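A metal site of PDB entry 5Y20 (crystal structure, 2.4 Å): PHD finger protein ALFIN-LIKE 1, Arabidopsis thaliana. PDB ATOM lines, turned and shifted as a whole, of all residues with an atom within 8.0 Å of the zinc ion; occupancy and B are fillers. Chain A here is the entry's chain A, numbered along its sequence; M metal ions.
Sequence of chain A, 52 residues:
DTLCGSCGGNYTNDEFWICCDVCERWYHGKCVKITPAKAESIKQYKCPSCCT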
ATOM      1  N   LEU A   3      -6.044   2.988  23.454  1.00  0.00           N
ATOM      2  CA  LEU A   3      -5.241   3.319  22.285  1.00  0.00           C
ATOM      3  C   LEU A   3      -3.801   2.930  22.535  1.00  0.00           C
ATOM      4  O   LEU A   3      -3.296   3.076  23.641  1.00  0.00           O
ATOM      5  CB  LEU A   3      -5.320   4.808  21.944  1.00  0.00           C
ATOM      6  CG  LEU A   3      -6.634   5.378  21.402  1.00  0.00           C
ATOM      7  CD1 LEU A   3      -6.415   6.821  21.019  1.00  0.00           C
ATOM      8  CD2 LEU A   3      -7.151   4.565  20.198  1.00  0.00           C
ATOM      9  N   CYS A   4      -3.151   2.431  21.493  1.00  0.00           N
ATOM     10  CA  CYS A   4      -1.782   1.980  21.580  1.00  0.00           C
ATOM     11  C   CYS A   4      -0.875   3.134  21.964  1.00  0.00           C
ATOM     12  O   CYS A   4      -0.880   4.184  21.322  1.00  0.00           O
ATOM     13  CB  CYS A   4      -1.345   1.372  20.253  1.00  0.00           C
ATOM     14  SG  CYS A   4       0.373   0.869  20.181  1.00  0.00           S
ATOM     15  N   GLY A   5      -0.085   2.923  23.017  1.00  0.00           N
ATOM     16  CA  GLY A   5       0.853   3.924  23.461  1.00  0.00           C
ATOM     17  C   GLY A   5       1.873   4.288  22.396  1.00  0.00           C
ATOM     18  O   GLY A   5       2.603   5.259  22.543  1.00  0.00           O
ATOM     19  N   SER A   6       1.921   3.518  21.320  1.00  0.00           N
ATOM     20  CA  SER A   6       2.935   3.720  20.301  1.00  0.00           C
ATOM     21  C   SER A   6       2.388   4.406  19.059  1.00  0.00           C
ATOM     22  O   SER A   6       2.891   5.453  18.655  1.00  0.00           O
ATOM     23  CB  SER A   6       3.555   2.376  19.913  1.00  0.00           C
ATOM     24  OG  SER A   6       4.663   2.573  19.071  1.00  0.00           O
ATOM     25  N   CYS A   7       1.365   3.810  18.457  1.00  0.00           N
ATOM     26  CA  CYS A   7       0.861   4.308  17.168  1.00  0.00           C
ATOM     27  C   CYS A   7      -0.478   5.025  17.305  1.00  0.00           C
ATOM     28  O   CYS A   7      -0.981   5.595  16.350  1.00  0.00           O
ATOM     29  CB  CYS A   7       0.710   3.152  16.179  1.00  0.00           C
ATOM     30  SG  CYS A   7      -0.530   1.941  16.673  1.00  0.00           S
ATOM     31  N   GLY A   8      -1.076   4.985  18.480  1.00  0.00           N
ATOM     32  CA  GLY A   8      -2.391   5.566  18.651  1.00  0.00           C
ATOM     33  C   GLY A   8      -3.522   4.708  18.121  1.00  0.00           C
ATOM     34  O   GLY A   8      -4.671   5.106  18.198  1.00  0.00           O
ATOM     35  N   GLY A   9      -3.209   3.526  17.582  1.00  0.00           N
ATOM     36  CA  GLY A   9      -4.222   2.642  17.043  1.00  0.00           C
ATOM     37  C   GLY A   9      -5.141   2.010  18.081  1.00  0.00           C
ATOM     38  O   GLY A   9      -4.766   1.851  19.231  1.00  0.00           O
ATOM     39  N   ASN A  10      -6.356   1.652  17.642  1.00  0.00           N
ATOM     40  CA  ASN A  10      -7.403   1.100  18.509  1.00  0.00           C
ATOM     41  C   ASN A  10      -7.184  -0.339  18.880  1.00  0.00           C
ATOM     42  O   ASN A  10      -6.633  -1.108  18.086  1.00  0.00           O
ATOM     43  CB  ASN A  10      -8.774   1.179  17.840  1.00  0.00           C
ATOM     44  CG  ASN A  10      -9.079   2.540  17.301  1.00  0.00           C
ATOM     45  OD1 ASN A  10      -8.618   2.900  16.220  1.00  0.00           O
ATOM     46  ND2 ASN A  10      -9.851   3.298  18.048  1.00  0.00           N
ATOM     47  N   PHE A  16      -2.442  -9.065  19.180  1.00  0.00           N
ATOM     48  CA  PHE A  16      -1.817  -9.289  20.476  1.00  0.00           C
ATOM     49  C   PHE A  16      -1.344  -7.965  21.055  1.00  0.00           C
ATOM     50  O   PHE A  16      -0.648  -7.201  20.388  1.00  0.00           O
ATOM     51  CB  PHE A  16      -0.649 -10.281  20.351  1.00  0.00           C
ATOM     52  CG  PHE A  16       0.233 -10.359  21.577  1.00  0.00           C
ATOM     53  CD1 PHE A  16      -0.211 -10.992  22.722  1.00  0.00           C
ATOM     54  CD2 PHE A  16       1.507  -9.815  21.565  1.00  0.00           C
ATOM     55  CE1 PHE A  16       0.602 -11.061  23.855  1.00  0.00           C
ATOM     56  CE2 PHE A  16       2.322  -9.878  22.690  1.00  0.00           C
ATOM     57  CZ  PHE A  16       1.868 -10.513  23.832  1.00  0.00           C
ATOM     58  N   TRP A  17      -1.757  -7.709  22.289  1.00  0.00           N
ATOM     59  CA  TRP A  17      -1.401  -6.510  23.025  1.00  0.00           C
ATOM     60  C   TRP A  17      -0.684  -6.875  24.318  1.00  0.00           C
ATOM     61  O   TRP A  17      -0.952  -7.916  24.925  1.00  0.00           O
ATOM     62  CB  TRP A  17      -2.642  -5.684  23.368  1.00  0.00           C
ATOM     63  CG  TRP A  17      -3.196  -4.915  22.245  1.00  0.00           C
ATOM     64  CD1 TRP A  17      -3.695  -5.414  21.069  1.00  0.00           C
ATOM     65  CD2 TRP A  17      -3.347  -3.497  22.177  1.00  0.00           C
ATOM     66  NE1 TRP A  17      -4.131  -4.383  20.268  1.00  0.00           N
ATOM     67  CE2 TRP A  17      -3.928  -3.199  20.921  1.00  0.00           C
ATOM     68  CE3 TRP A  17      -3.042  -2.442  23.048  1.00  0.00           C
ATOM     69  CZ2 TRP A  17      -4.192  -1.883  20.521  1.00  0.00           C
ATOM     70  CZ3 TRP A  17      -3.299  -1.147  22.644  1.00  0.00           C
ATOM     71  CH2 TRP A  17      -3.884  -0.879  21.389  1.00  0.00           C
ATOM     72  N   TRP A  26      -0.645   0.502  27.440  1.00  0.00           N
ATOM     73  CA  TRP A  26      -0.950  -0.668  26.629  1.00  0.00           C
ATOM     74  C   TRP A  26      -0.427  -0.497  25.216  1.00  0.00           C
ATOM     75  O   TRP A  26      -0.510   0.592  24.648  1.00  0.00           O
ATOM     76  CB  TRP A  26      -2.449  -0.942  26.618  1.00  0.00           C
ATOM     77  CG  TRP A  26      -2.890  -1.775  27.779  1.00  0.00           C
ATOM     78  CD1 TRP A  26      -3.481  -1.326  28.943  1.00  0.00           C
ATOM     79  CD2 TRP A  26      -2.763  -3.189  27.913  1.00  0.00           C
ATOM     80  NE1 TRP A  26      -3.740  -2.397  29.773  1.00  0.00           N
ATOM     81  CE2 TRP A  26      -3.305  -3.548  29.169  1.00  0.00           C
ATOM     82  CE3 TRP A  26      -2.258  -4.205  27.092  1.00  0.00           C
ATOM     83  CZ2 TRP A  26      -3.348  -4.858  29.604  1.00  0.00           C
ATOM     84  CZ3 TRP A  26      -2.295  -5.505  27.535  1.00  0.00           C
ATOM     85  CH2 TRP A  26      -2.841  -5.824  28.772  1.00  0.00           C
ATOM     86  N   TYR A  27       0.111  -1.572  24.635  1.00  0.00           N
ATOM     87  CA  TYR A  27       0.729  -1.505  23.315  1.00  0.00           C
ATOM     88  C   TYR A  27       0.303  -2.652  22.393  1.00  0.00           C
ATOM     89  O   TYR A  27       0.062  -3.756  22.870  1.00  0.00           O
ATOM     90  CB  TYR A  27       2.238  -1.559  23.421  1.00  0.00           C
ATOM     91  CG  TYR A  27       2.922  -0.406  24.118  1.00  0.00           C
ATOM     92  CD1 TYR A  27       3.284   0.728  23.418  1.00  0.00           C
ATOM     93  CD2 TYR A  27       3.262  -0.478  25.468  1.00  0.00           C
ATOM     94  CE1 TYR A  27       3.940   1.784  24.045  1.00  0.00           C
ATOM     95  CE2 TYR A  27       3.925   0.558  26.091  1.00  0.00           C
ATOM     96  CZ  TYR A  27       4.260   1.690  25.374  1.00  0.00           C
ATOM     97  OH  TYR A  27       4.915   2.730  25.986  1.00  0.00           O
ATOM     98  N   HIS A  28       0.235  -2.392  21.087  1.00  0.00           N
ATOM     99  CA  HIS A  28       0.301  -3.466  20.100  1.00  0.00           C
ATOM    100  C   HIS A  28       1.575  -4.239  20.365  1.00  0.00           C
ATOM    101  O   HIS A  28       2.628  -3.620  20.532  1.00  0.00           O
ATOM    102  CB  HIS A  28       0.351  -2.952  18.667  1.00  0.00           C
ATOM    103  CG  HIS A  28      -0.963  -2.500  18.118  1.00  0.00           C
ATOM    104  ND1 HIS A  28      -1.187  -1.198  17.710  1.00  0.00           N
ATOM    105  CD2 HIS A  28      -2.105  -3.165  17.863  1.00  0.00           C
ATOM    106  CE1 HIS A  28      -2.416  -1.089  17.240  1.00  0.00           C
ATOM    107  NE2 HIS A  28      -2.995  -2.271  17.326  1.00  0.00           N
ATOM    108  N   GLY A  29       1.503  -5.562  20.408  1.00  0.00           N
ATOM    109  CA  GLY A  29       2.706  -6.368  20.455  1.00  0.00           C
ATOM    110  C   GLY A  29       3.594  -6.043  19.263  1.00  0.00           C
ATOM    111  O   GLY A  29       4.828  -6.025  19.358  1.00  0.00           O
ATOM    112  N   LYS A  30       2.970  -5.774  18.122  1.00  0.00           N
ATOM    113  CA  LYS A  30       3.711  -5.477  16.903  1.00  0.00           C
ATOM    114  C   LYS A  30       4.468  -4.158  16.989  1.00  0.00           C
ATOM    115  O   LYS A  30       5.549  -4.030  16.414  1.00  0.00           O
ATOM    116  CB  LYS A  30       2.763  -5.450  15.718  1.00  0.00           C
ATOM    117  CG  LYS A  30       2.294  -6.798  15.277  1.00  0.00           C
ATOM    118  CD  LYS A  30       1.252  -6.677  14.172  1.00  0.00           C
ATOM    119  CE  LYS A  30       0.822  -8.043  13.693  1.00  0.00           C
ATOM    120  NZ  LYS A  30      -0.361  -7.969  12.820  1.00  0.00           N
ATOM    121  N   CYS A  31       3.917  -3.178  17.685  1.00  0.00           N
ATOM    122  CA  CYS A  31       4.589  -1.889  17.789  1.00  0.00           C
ATOM    123  C   CYS A  31       5.823  -1.959  18.671  1.00  0.00           C
ATOM    124  O   CYS A  31       6.864  -1.389  18.327  1.00  0.00           O
ATOM    125  CB  CYS A  31       3.638  -0.822  18.314  1.00  0.00           C
ATOM    126  SG  CYS A  31       2.423  -0.383  17.088  1.00  0.00           S
ATOM    127  N   VAL A  32       5.730  -2.666  19.796  1.00  0.00           N
ATOM    128  CA  VAL A  32       6.880  -2.796  20.683  1.00  0.00           C
ATOM    129  C   VAL A  32       7.685  -4.071  20.400  1.00  0.00           C
ATOM    130  O   VAL A  32       8.669  -4.353  21.090  1.00  0.00           O
ATOM    131  CB  VAL A  32       6.458  -2.776  22.164  1.00  0.00           C
ATOM    132  CG1 VAL A  32       5.902  -1.387  22.520  1.00  0.00           C
ATOM    133  CG2 VAL A  32       5.435  -3.860  22.463  1.00  0.00           C
HETATM  134 ZN    ZN M   1       0.426   0.195  17.972  1.00  0.00          ZN
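SG of Cys 4 lies close to N of Ser 6, 3.3 Å away.
The backbone NH of Cys 4 is in hydrogen-bond range of the backbone carbonyl oxygen of Gly 9.
SG of Cys 7 sits close to N of Gly 9.
The zinc ion is bound by a ring nitrogen (ND1) of His 28, the side-chain sulfur (SG) of Cys 31, the side-chain sulfur (SG) of Cys 4 and the side-chain sulfur (SG) of Cys 7.
The zinc ion has four donor atoms within binding distance.
Of the 17 residues printed, 4 come within 4 Å of the zinc ion.
The nearest printed residue that does not touch the zinc ion is Ser 6 (4.3 Å).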
